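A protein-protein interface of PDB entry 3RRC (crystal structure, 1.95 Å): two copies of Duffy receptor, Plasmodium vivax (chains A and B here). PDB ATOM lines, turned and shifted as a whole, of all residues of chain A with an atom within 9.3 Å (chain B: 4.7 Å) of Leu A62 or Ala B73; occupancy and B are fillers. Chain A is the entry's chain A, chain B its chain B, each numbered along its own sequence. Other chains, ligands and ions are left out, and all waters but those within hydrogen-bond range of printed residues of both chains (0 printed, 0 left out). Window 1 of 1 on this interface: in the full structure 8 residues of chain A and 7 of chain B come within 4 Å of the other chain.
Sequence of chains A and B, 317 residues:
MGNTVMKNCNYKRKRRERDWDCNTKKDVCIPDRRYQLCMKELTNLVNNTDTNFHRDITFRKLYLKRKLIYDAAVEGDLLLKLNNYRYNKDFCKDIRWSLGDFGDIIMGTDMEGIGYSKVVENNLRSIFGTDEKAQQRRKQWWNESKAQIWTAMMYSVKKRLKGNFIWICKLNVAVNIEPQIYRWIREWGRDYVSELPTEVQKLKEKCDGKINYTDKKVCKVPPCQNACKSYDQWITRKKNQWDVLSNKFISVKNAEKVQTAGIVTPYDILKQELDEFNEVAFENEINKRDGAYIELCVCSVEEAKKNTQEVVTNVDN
The side-chain hydroxyl of Tyr B155 is in hydrogen-bond range of the side-chain hydroxyl of Thr A58, 3.0 Å away.
The side-chain hydroxyl (OG1) of Thr A58 lies close to the backbone NH (N) of Arg A60 (3.1 Å).
OG1 of Thr A58 lies within hydrogen-bond range of N of Lys A61 (3.0 Å).
Among the printed residues, pairs that only touch across the chains: Phe A59 with Ala B73 (3.5 Å), Arg A66 with Tyr B70 (3.5 Å), Leu A62 with Ala B73 (3.5 Å), Phe A59 with Tyr B155 (3.7 Å), Lys A61 with Tyr B155 (3.7 Å), Phe A59 with Asp B77 (3.8 Å) and Phe A59 with Tyr B70 (3.998 Å).
Of the printed residues of chain B, Lys A61 touches Tyr B155 (3.7 Å).
Printed residues of chain B within 4 Å of Leu A62: Ala B73 (3.5 Å).
Ile B69 touches none of the printed residues of chain A.
Of the printed residues of chain A, Tyr B70 touches Phe A59 (3.998 Å) and Arg A66 (3.5 Å).
Asp B71 touches none of the printed residues of chain A.
No residue of chain A comes within 4 Å of Ala B72.
Ala B73 touches just these residues of chain A: Phe A59 and Leu A62.
Val B74 touches none of the printed residues of chain A.
No residue of chain A comes within 4 Å of Gly B76.
Printed residues of chain A within 4 Å of Asp B77: Phe A59 (3.8 Å).
The nearest printed residue of chain B that does not touch Leu A62 is Ile B69 (4.01 Å).
The nearest residue of chain A that does not touch Ala B73 is Thr A58 (8.4 Å).
The nearest printed residue of chain B that does not touch Arg A66 is Ile B69 (6.5 Å).
Hydrophobic or aromatic side chains of chain A within 4 Å of the printed part of chain B: Phe A59 and Leu A62.
Printed residues of chain B that touch a printed residue of chain A: Tyr B70, Ala B73, Asp B77 and Tyr B155.
Among the printed residues, no Asp or Glu carboxylate lies within 4 Å of a Lys or Arg side-chain nitrogen of the other chain.
1 position is printed for both chains.
Of the 8 pairs that touch across the chains among the printed residues, none has its exchanged pair printed and touching as well.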
ATOM      1  N   LEU A  45      -8.571 -23.850 -18.943  1.00  0.00           N
ATOM      2  CA  LEU A  45      -8.988 -23.440 -17.616  1.00  0.00           C
ATOM      3  C   LEU A  45     -10.446 -23.806 -17.358  1.00  0.00           C
ATOM      4  O   LEU A  45     -10.969 -24.757 -17.936  1.00  0.00           O
ATOM      5  CB  LEU A  45      -8.789 -21.933 -17.486  1.00  0.00           C
ATOM      6  CG  LEU A  45      -9.045 -21.301 -16.126  1.00  0.00           C
ATOM      7  CD1 LEU A  45      -8.128 -21.904 -15.085  1.00  0.00           C
ATOM      8  CD2 LEU A  45      -8.849 -19.801 -16.214  1.00  0.00           C
ATOM      9  N   THR A  58     -13.465 -18.786  -3.728  1.00  0.00           N
ATOM     10  CA  THR A  58     -13.460 -19.326  -5.073  1.00  0.00           C
ATOM     11  C   THR A  58     -12.288 -20.283  -5.226  1.00  0.00           C
ATOM     12  O   THR A  58     -12.451 -21.445  -5.602  1.00  0.00           O
ATOM     13  CB  THR A  58     -13.332 -18.188  -6.128  1.00  0.00           C
ATOM     14  OG1 THR A  58     -11.984 -17.686  -6.161  1.00  0.00           O
ATOM     15  CG2 THR A  58     -14.269 -17.048  -5.791  1.00  0.00           C
ATOM     16  N   PHE A  59     -11.111 -19.777  -4.883  1.00  0.00           N
ATOM     17  CA  PHE A  59      -9.852 -20.281  -5.403  1.00  0.00           C
ATOM     18  C   PHE A  59      -9.775 -20.184  -6.939  1.00  0.00           C
ATOM     19  O   PHE A  59      -8.684 -20.091  -7.463  1.00  0.00           O
ATOM     20  CB  PHE A  59      -9.545 -21.701  -4.947  1.00  0.00           C
ATOM     21  CG  PHE A  59      -9.250 -21.814  -3.466  1.00  0.00           C
ATOM     22  CD1 PHE A  59      -8.876 -20.702  -2.730  1.00  0.00           C
ATOM     23  CD2 PHE A  59      -9.350 -23.034  -2.818  1.00  0.00           C
ATOM     24  CE1 PHE A  59      -8.611 -20.808  -1.370  1.00  0.00           C
ATOM     25  CE2 PHE A  59      -9.092 -23.139  -1.460  1.00  0.00           C
ATOM     26  CZ  PHE A  59      -8.723 -22.023  -0.740  1.00  0.00           C
ATOM     27  N   ARG A  60     -10.904 -20.225  -7.649  1.00  0.00           N
ATOM     28  CA  ARG A  60     -10.871 -20.099  -9.113  1.00  0.00           C
ATOM     29  C   ARG A  60     -10.293 -18.758  -9.545  1.00  0.00           C
ATOM     30  O   ARG A  60      -9.602 -18.679 -10.559  1.00  0.00           O
ATOM     31  CB  ARG A  60     -12.262 -20.299  -9.723  1.00  0.00           C
ATOM     32  CG  ARG A  60     -12.806 -21.717  -9.538  1.00  0.00           C
ATOM     33  CD  ARG A  60     -14.315 -21.784  -9.725  1.00  0.00           C
ATOM     34  NE  ARG A  60     -14.688 -22.091 -11.098  1.00  0.00           N
ATOM     35  CZ  ARG A  60     -15.926 -21.998 -11.572  1.00  0.00           C
ATOM     36  NH1 ARG A  60     -16.915 -21.599 -10.781  1.00  0.00           N
ATOM     37  NH2 ARG A  60     -16.172 -22.296 -12.843  1.00  0.00           N
ATOM     38  N   LYS A  61     -10.581 -17.694  -8.806  1.00  0.00           N
ATOM     39  CA  LYS A  61     -10.002 -16.393  -9.158  1.00  0.00           C
ATOM     40  C   LYS A  61      -8.493 -16.362  -8.932  1.00  0.00           C
ATOM     41  O   LYS A  61      -7.769 -15.745  -9.710  1.00  0.00           O
ATOM     42  CB  LYS A  61     -10.699 -15.257  -8.418  1.00  0.00           C
ATOM     43  CG  LYS A  61     -12.120 -15.061  -8.901  1.00  0.00           C
ATOM     44  CD  LYS A  61     -12.783 -13.847  -8.291  1.00  0.00           C
ATOM     45  CE  LYS A  61     -14.243 -13.784  -8.704  1.00  0.00           C
ATOM     46  NZ  LYS A  61     -15.009 -14.974  -8.224  1.00  0.00           N
ATOM     47  N   LEU A  62      -8.013 -17.034  -7.881  1.00  0.00           N
ATOM     48  CA  LEU A  62      -6.578 -17.131  -7.643  1.00  0.00           C
ATOM     49  C   LEU A  62      -5.945 -17.959  -8.738  1.00  0.00           C
ATOM     50  O   LEU A  62      -4.834 -17.679  -9.171  1.00  0.00           O
ATOM     51  CB  LEU A  62      -6.238 -17.791  -6.284  1.00  0.00           C
ATOM     52  CG  LEU A  62      -6.469 -16.986  -5.006  1.00  0.00           C
ATOM     53  CD1 LEU A  62      -6.114 -17.836  -3.763  1.00  0.00           C
ATOM     54  CD2 LEU A  62      -5.661 -15.695  -5.028  1.00  0.00           C
ATOM     55  N   TYR A  63      -6.639 -19.007  -9.152  1.00  0.00           N
ATOM     56  CA  TYR A  63      -6.125 -19.880 -10.186  1.00  0.00           C
ATOM     57  C   TYR A  63      -6.086 -19.098 -11.510  1.00  0.00           C
ATOM     58  O   TYR A  63      -5.124 -19.199 -12.271  1.00  0.00           O
ATOM     59  CB  TYR A  63      -6.988 -21.142 -10.294  1.00  0.00           C
ATOM     60  CG  TYR A  63      -6.346 -22.267 -11.082  1.00  0.00           C
ATOM     61  CD1 TYR A  63      -5.205 -22.913 -10.616  1.00  0.00           C
ATOM     62  CD2 TYR A  63      -6.883 -22.687 -12.291  1.00  0.00           C
ATOM     63  CE1 TYR A  63      -4.616 -23.943 -11.342  1.00  0.00           C
ATOM     64  CE2 TYR A  63      -6.305 -23.713 -13.021  1.00  0.00           C
ATOM     65  CZ  TYR A  63      -5.174 -24.338 -12.543  1.00  0.00           C
ATOM     66  OH  TYR A  63      -4.602 -25.357 -13.271  1.00  0.00           O
ATOM     67  N   LEU A  64      -7.118 -18.292 -11.746  1.00  0.00           N
ATOM     68  CA  LEU A  64      -7.176 -17.432 -12.928  1.00  0.00           C
ATOM     69  C   LEU A  64      -5.953 -16.527 -13.020  1.00  0.00           C
ATOM     70  O   LEU A  64      -5.323 -16.430 -14.077  1.00  0.00           O
ATOM     71  CB  LEU A  64      -8.444 -16.567 -12.916  1.00  0.00           C
ATOM     72  CG  LEU A  64      -8.503 -15.502 -14.034  1.00  0.00           C
ATOM     73  CD1 LEU A  64      -8.247 -16.117 -15.390  1.00  0.00           C
ATOM     74  CD2 LEU A  64      -9.834 -14.777 -14.029  1.00  0.00           C
ATOM     75  N   LYS A  65      -5.619 -15.860 -11.924  1.00  0.00           N
ATOM     76  CA  LYS A  65      -4.501 -14.929 -11.930  1.00  0.00           C
ATOM     77  C   LYS A  65      -3.196 -15.638 -12.261  1.00  0.00           C
ATOM     78  O   LYS A  65      -2.368 -15.094 -12.986  1.00  0.00           O
ATOM     79  CB  LYS A  65      -4.385 -14.189 -10.599  1.00  0.00           C
ATOM     80  CG  LYS A  65      -3.363 -13.063 -10.640  1.00  0.00           C
ATOM     81  CD  LYS A  65      -3.543 -12.108  -9.483  1.00  0.00           C
ATOM     82  CE  LYS A  65      -4.254 -10.834  -9.913  1.00  0.00           C
ATOM     83  NZ  LYS A  65      -4.484  -9.896  -8.770  1.00  0.00           N
ATOM     84  N   ARG A  66      -2.990 -16.833 -11.710  1.00  0.00           N
ATOM     85  CA  ARG A  66      -1.814 -17.624 -12.065  1.00  0.00           C
ATOM     86  C   ARG A  66      -1.794 -17.953 -13.560  1.00  0.00           C
ATOM     87  O   ARG A  66      -0.758 -17.836 -14.202  1.00  0.00           O
ATOM     88  CB  ARG A  66      -1.735 -18.922 -11.263  1.00  0.00           C
ATOM     89  CG  ARG A  66      -0.703 -18.836 -10.199  1.00  0.00           C
ATOM     90  CD  ARG A  66       0.217 -20.049 -10.170  1.00  0.00           C
ATOM     91  NE  ARG A  66      -0.473 -21.341 -10.115  1.00  0.00           N
ATOM     92  CZ  ARG A  66      -1.367 -21.697  -9.192  1.00  0.00           C
ATOM     93  NH1 ARG A  66      -1.712 -20.869  -8.216  1.00  0.00           N
ATOM     94  NH2 ARG A  66      -1.922 -22.899  -9.246  1.00  0.00           N
ATOM     95  N   LYS A  67      -2.941 -18.341 -14.109  1.00  0.00           N
ATOM     96  CA  LYS A  67      -3.016 -18.776 -15.492  1.00  0.00           C
ATOM     97  C   LYS A  67      -2.770 -17.604 -16.441  1.00  0.00           C
ATOM     98  O   LYS A  67      -2.168 -17.777 -17.495  1.00  0.00           O
ATOM     99  CB  LYS A  67      -4.360 -19.464 -15.756  1.00  0.00           C
ATOM    100  CG  LYS A  67      -4.465 -20.847 -15.109  1.00  0.00           C
ATOM    101  CD  LYS A  67      -3.089 -21.532 -15.093  1.00  0.00           C
ATOM    102  CE  LYS A  67      -3.118 -22.901 -14.445  1.00  0.00           C
ATOM    103  NZ  LYS A  67      -1.737 -23.424 -14.223  1.00  0.00           N
ATOM    104  N   LEU A  68      -3.216 -16.417 -16.040  1.00  0.00           N
ATOM    105  CA  LEU A  68      -3.102 -15.223 -16.855  1.00  0.00           C
ATOM    106  C   LEU A  68      -1.670 -14.709 -16.808  1.00  0.00           C
ATOM    107  O   LEU A  68      -1.174 -14.138 -17.779  1.00  0.00           O
ATOM    108  CB  LEU A  68      -4.067 -14.139 -16.362  1.00  0.00           C
ATOM    109  CG  LEU A  68      -4.004 -12.808 -17.122  1.00  0.00           C
ATOM    110  CD1 LEU A  68      -4.328 -12.995 -18.596  1.00  0.00           C
ATOM    111  CD2 LEU A  68      -4.936 -11.783 -16.513  1.00  0.00           C
ATOM    112  N   ILE A  69      -1.005 -14.920 -15.674  1.00  0.00           N
ATOM    113  CA  ILE A  69       0.381 -14.508 -15.510  1.00  0.00           C
ATOM    114  C   ILE A  69       1.269 -15.376 -16.390  1.00  0.00           C
ATOM    115  O   ILE A  69       2.185 -14.871 -17.019  1.00  0.00           O
ATOM    116  CB  ILE A  69       0.841 -14.584 -14.022  1.00  0.00           C
ATOM    117  CG1 ILE A  69       0.255 -13.406 -13.235  1.00  0.00           C
ATOM    118  CG2 ILE A  69       2.380 -14.581 -13.906  1.00  0.00           C
ATOM    119  CD1 ILE A  69       0.460 -13.492 -11.755  1.00  0.00           C
ATOM    120  N   ILE A 127     -16.566 -18.329 -14.178  1.00  0.00           N
ATOM    121  CA  ILE A 127     -15.837 -17.865 -13.004  1.00  0.00           C
ATOM    122  C   ILE A 127     -16.499 -16.645 -12.364  1.00  0.00           C
ATOM    123  O   ILE A 127     -16.594 -16.564 -11.145  1.00  0.00           O
ATOM    124  CB  ILE A 127     -14.364 -17.534 -13.333  1.00  0.00           C
ATOM    125  CG1 ILE A 127     -13.578 -18.808 -13.641  1.00  0.00           C
ATOM    126  CG2 ILE A 127     -13.696 -16.814 -12.170  1.00  0.00           C
ATOM    127  CD1 ILE A 127     -12.191 -18.520 -14.224  1.00  0.00           C
ATOM    128  N   PHE A 128     -16.960 -15.703 -13.180  1.00  0.00           N
ATOM    129  CA  PHE A 128     -17.436 -14.420 -12.668  1.00  0.00           C
ATOM    130  C   PHE A 128     -18.964 -14.307 -12.670  1.00  0.00           C
ATOM    131  O   PHE A 128     -19.534 -13.488 -11.948  1.00  0.00           O
ATOM    132  CB  PHE A 128     -16.854 -13.263 -13.492  1.00  0.00           C
ATOM    133  CG  PHE A 128     -15.386 -12.997 -13.240  1.00  0.00           C
ATOM    134  CD1 PHE A 128     -14.990 -12.085 -12.275  1.00  0.00           C
ATOM    135  CD2 PHE A 128     -14.411 -13.636 -13.992  1.00  0.00           C
ATOM    136  CE1 PHE A 128     -13.648 -11.826 -12.043  1.00  0.00           C
ATOM    137  CE2 PHE A 128     -13.064 -13.383 -13.773  1.00  0.00           C
ATOM    138  CZ  PHE A 128     -12.680 -12.475 -12.794  1.00  0.00           C
ATOM    139  N   TRP A 141     -11.629  -6.428 -11.419  1.00  0.00           N
ATOM    140  CA  TRP A 141     -10.562  -7.407 -11.246  1.00  0.00           C
ATOM    141  C   TRP A 141      -9.382  -7.088 -12.177  1.00  0.00           C
ATOM    142  O   TRP A 141      -8.221  -7.262 -11.806  1.00  0.00           O
ATOM    143  CB  TRP A 141     -11.105  -8.813 -11.506  1.00  0.00           C
ATOM    144  CG  TRP A 141     -10.152  -9.931 -11.208  1.00  0.00           C
ATOM    145  CD1 TRP A 141     -10.013 -10.605 -10.018  1.00  0.00           C
ATOM    146  CD2 TRP A 141      -9.213 -10.528 -12.113  1.00  0.00           C
ATOM    147  NE1 TRP A 141      -9.041 -11.569 -10.134  1.00  0.00           N
ATOM    148  CE2 TRP A 141      -8.540 -11.547 -11.408  1.00  0.00           C
ATOM    149  CE3 TRP A 141      -8.878 -10.301 -13.451  1.00  0.00           C
ATOM    150  CZ2 TRP A 141      -7.554 -12.332 -11.997  1.00  0.00           C
ATOM    151  CZ3 TRP A 141      -7.892 -11.080 -14.028  1.00  0.00           C
ATOM    152  CH2 TRP A 141      -7.246 -12.085 -13.304  1.00  0.00           C
ATOM    153  N   SER A 145      -5.335  -6.090 -11.382  1.00  0.00           N
ATOM    154  CA  SER A 145      -4.385  -7.101 -11.821  1.00  0.00           C
ATOM    155  C   SER A 145      -3.437  -6.630 -12.917  1.00  0.00           C
ATOM    156  O   SER A 145      -2.397  -7.251 -13.143  1.00  0.00           O
ATOM    157  CB  SER A 145      -5.144  -8.336 -12.299  1.00  0.00           C
ATOM    158  OG  SER A 145      -6.064  -8.771 -11.310  1.00  0.00           O
ATOM    159  N   GLN A 148       0.412  -6.298 -12.559  1.00  0.00           N
ATOM    160  CA  GLN A 148       1.130  -7.553 -12.376  1.00  0.00           C
ATOM    161  C   GLN A 148       1.295  -8.263 -13.696  1.00  0.00           C
ATOM    162  O   GLN A 148       2.304  -8.921 -13.947  1.00  0.00           O
ATOM    163  CB  GLN A 148       0.344  -8.475 -11.424  1.00  0.00           C
ATOM    164  CG  GLN A 148       0.430  -8.102  -9.960  1.00  0.00           C
ATOM    165  CD  GLN A 148      -0.622  -8.825  -9.133  1.00  0.00           C
ATOM    166  OE1 GLN A 148      -1.821  -8.689  -9.382  1.00  0.00           O
ATOM    167  NE2 GLN A 148      -0.176  -9.617  -8.159  1.00  0.00           N
ATOM    168  N   ILE B  69       1.107 -17.855  -2.449  1.00  0.00           N
ATOM    169  CA  ILE B  69      -0.209 -17.312  -2.136  1.00  0.00           C
ATOM    170  C   ILE B  69      -1.231 -18.433  -2.225  1.00  0.00           C
ATOM    171  O   ILE B  69      -2.141 -18.508  -1.411  1.00  0.00           O
ATOM    172  CB  ILE B  69      -0.590 -16.124  -3.077  1.00  0.00           C
ATOM    173  CG1 ILE B  69       0.039 -14.825  -2.563  1.00  0.00           C
ATOM    174  CG2 ILE B  69      -2.111 -15.968  -3.191  1.00  0.00           C
ATOM    175  CD1 ILE B  69      -0.122 -13.630  -3.487  1.00  0.00           C
ATOM    176  N   TYR B  70      -1.064 -19.324  -3.195  1.00  0.00           N
ATOM    177  CA  TYR B  70      -2.022 -20.399  -3.373  1.00  0.00           C
ATOM    178  C   TYR B  70      -1.930 -21.431  -2.245  1.00  0.00           C
ATOM    179  O   TYR B  70      -2.947 -21.915  -1.754  1.00  0.00           O
ATOM    180  CB  TYR B  70      -1.845 -21.102  -4.716  1.00  0.00           C
ATOM    181  CG  TYR B  70      -3.083 -21.895  -5.089  1.00  0.00           C
ATOM    182  CD1 TYR B  70      -4.200 -21.259  -5.621  1.00  0.00           C
ATOM    183  CD2 TYR B  70      -3.148 -23.268  -4.888  1.00  0.00           C
ATOM    184  CE1 TYR B  70      -5.341 -21.970  -5.950  1.00  0.00           C
ATOM    185  CE2 TYR B  70      -4.291 -23.990  -5.212  1.00  0.00           C
ATOM    186  CZ  TYR B  70      -5.379 -23.335  -5.748  1.00  0.00           C
ATOM    187  OH  TYR B  70      -6.513 -24.049  -6.079  1.00  0.00           O
ATOM    188  N   ASP B  71      -0.712 -21.777  -1.858  1.00  0.00           N
ATOM    189  CA  ASP B  71      -0.503 -22.728  -0.767  1.00  0.00           C
ATOM    190  C   ASP B  71      -1.063 -22.163   0.552  1.00  0.00           C
ATOM    191  O   ASP B  71      -1.726 -22.862   1.314  1.00  0.00           O
ATOM    192  CB  ASP B  71       0.985 -23.023  -0.619  1.00  0.00           C
ATOM    193  CG  ASP B  71       1.475 -24.127  -1.564  1.00  0.00           C
ATOM    194  OD1 ASP B  71       0.666 -24.970  -2.023  1.00  0.00           O
ATOM    195  OD2 ASP B  71       2.695 -24.161  -1.837  1.00  0.00           O
ATOM    196  N   ALA B  72      -0.783 -20.893   0.799  1.00  0.00           N
ATOM    197  CA  ALA B  72      -1.279 -20.201   1.971  1.00  0.00           C
ATOM    198  C   ALA B  72      -2.811 -20.137   1.961  1.00  0.00           C
ATOM    199  O   ALA B  72      -3.455 -20.320   2.986  1.00  0.00           O
ATOM    200  CB  ALA B  72      -0.679 -18.777   2.041  1.00  0.00           C
ATOM    201  N   ALA B  73      -3.403 -19.866   0.805  1.00  0.00           N
ATOM    202  CA  ALA B  73      -4.856 -19.827   0.729  1.00  0.00           C
ATOM    203  C   ALA B  73      -5.448 -21.211   1.053  1.00  0.00           C
ATOM    204  O   ALA B  73      -6.446 -21.330   1.775  1.00  0.00           O
ATOM    205  CB  ALA B  73      -5.316 -19.333  -0.677  1.00  0.00           C
ATOM    206  N   VAL B  74      -4.829 -22.261   0.533  1.00  0.00           N
ATOM    207  CA  VAL B  74      -5.315 -23.608   0.808  1.00  0.00           C
ATOM    208  C   VAL B  74      -5.126 -23.917   2.326  1.00  0.00           C
ATOM    209  O   VAL B  74      -6.016 -24.451   2.985  1.00  0.00           O
ATOM    210  CB  VAL B  74      -4.584 -24.653  -0.081  1.00  0.00           C
ATOM    211  CG1 VAL B  74      -4.919 -26.060   0.372  1.00  0.00           C
ATOM    212  CG2 VAL B  74      -4.965 -24.456  -1.580  1.00  0.00           C
ATOM    213  N   GLU B  75      -3.978 -23.536   2.872  1.00  0.00           N
ATOM    214  CA  GLU B  75      -3.650 -23.790   4.295  1.00  0.00           C
ATOM    215  C   GLU B  75      -4.675 -23.112   5.207  1.00  0.00           C
ATOM    216  O   GLU B  75      -5.156 -23.706   6.185  1.00  0.00           O
ATOM    217  CB  GLU B  75      -2.227 -23.270   4.630  1.00  0.00           C
ATOM    218  CG  GLU B  75      -1.844 -23.410   6.131  1.00  0.00           C
ATOM    219  CD  GLU B  75      -1.615 -24.849   6.574  1.00  0.00           C
ATOM    220  OE1 GLU B  75      -1.630 -25.751   5.701  1.00  0.00           O
ATOM    221  OE2 GLU B  75      -1.412 -25.081   7.799  1.00  0.00           O
ATOM    222  N   GLY B  76      -4.994 -21.866   4.869  1.00  0.00           N
ATOM    223  CA  GLY B  76      -5.914 -21.050   5.630  1.00  0.00           C
ATOM    224  C   GLY B  76      -7.308 -21.659   5.638  1.00  0.00           C
ATOM    225  O   GLY B  76      -7.941 -21.736   6.694  1.00  0.00           O
ATOM    226  N   ASP B  77      -7.779 -22.094   4.467  1.00  0.00           N
ATOM    227  CA  ASP B  77      -9.114 -22.693   4.337  1.00  0.00           C
ATOM    228  C   ASP B  77      -9.205 -24.006   5.136  1.00  0.00           C
ATOM    229  O   ASP B  77     -10.204 -24.271   5.803  1.00  0.00           O
ATOM    230  CB  ASP B  77      -9.418 -22.976   2.871  1.00  0.00           C
ATOM    231  CG  ASP B  77     -10.800 -23.529   2.673  1.00  0.00           C
ATOM    232  OD1 ASP B  77     -11.736 -22.878   3.151  1.00  0.00           O
ATOM    233  OD2 ASP B  77     -10.948 -24.614   2.078  1.00  0.00           O
ATOM    234  N   ALA B 152      -3.801 -13.832   1.913  1.00  0.00           N
ATOM    235  CA  ALA B 152      -4.068 -15.066   1.192  1.00  0.00           C
ATOM    236  C   ALA B 152      -4.580 -16.150   2.155  1.00  0.00           C
ATOM    237  O   ALA B 152      -5.560 -16.814   1.854  1.00  0.00           O
ATOM    238  CB  ALA B 152      -2.797 -15.546   0.462  1.00  0.00           C
ATOM    239  N   MET B 153      -3.938 -16.342   3.310  1.00  0.00           N
ATOM    240  CA  MET B 153      -4.466 -17.334   4.237  1.00  0.00           C
ATOM    241  C   MET B 153      -5.897 -17.017   4.637  1.00  0.00           C
ATOM    242  O   MET B 153      -6.677 -17.931   4.909  1.00  0.00           O
ATOM    243  CB  MET B 153      -3.613 -17.473   5.497  1.00  0.00           C
ATOM    244  CG  MET B 153      -2.188 -17.898   5.194  1.00  0.00           C
ATOM    245  SD  MET B 153      -1.219 -18.220   6.681  1.00  0.00           S
ATOM    246  CE  MET B 153      -1.966 -19.730   7.246  1.00  0.00           C
ATOM    247  N   TYR B 155      -8.101 -15.813   2.706  1.00  0.00           N
ATOM    248  CA  TYR B 155      -8.932 -15.723   1.492  1.00  0.00           C
ATOM    249  C   TYR B 155     -10.303 -16.367   1.720  1.00  0.00           C
ATOM    250  O   TYR B 155     -11.323 -15.864   1.266  1.00  0.00           O
ATOM    251  CB  TYR B 155      -8.227 -16.394   0.310  1.00  0.00           C
ATOM    252  CG  TYR B 155      -8.868 -16.119  -1.033  1.00  0.00           C
ATOM    253  CD1 TYR B 155      -8.670 -14.910  -1.682  1.00  0.00           C
ATOM    254  CD2 TYR B 155      -9.658 -17.076  -1.659  1.00  0.00           C
ATOM    255  CE1 TYR B 155      -9.247 -14.657  -2.916  1.00  0.00           C
ATOM    256  CE2 TYR B 155     -10.240 -16.833  -2.885  1.00  0.00           C
ATOM    257  CZ  TYR B 155     -10.025 -15.625  -3.512  1.00  0.00           C
ATOM    258  OH  TYR B 155     -10.606 -15.381  -4.732  1.00  0.00           O
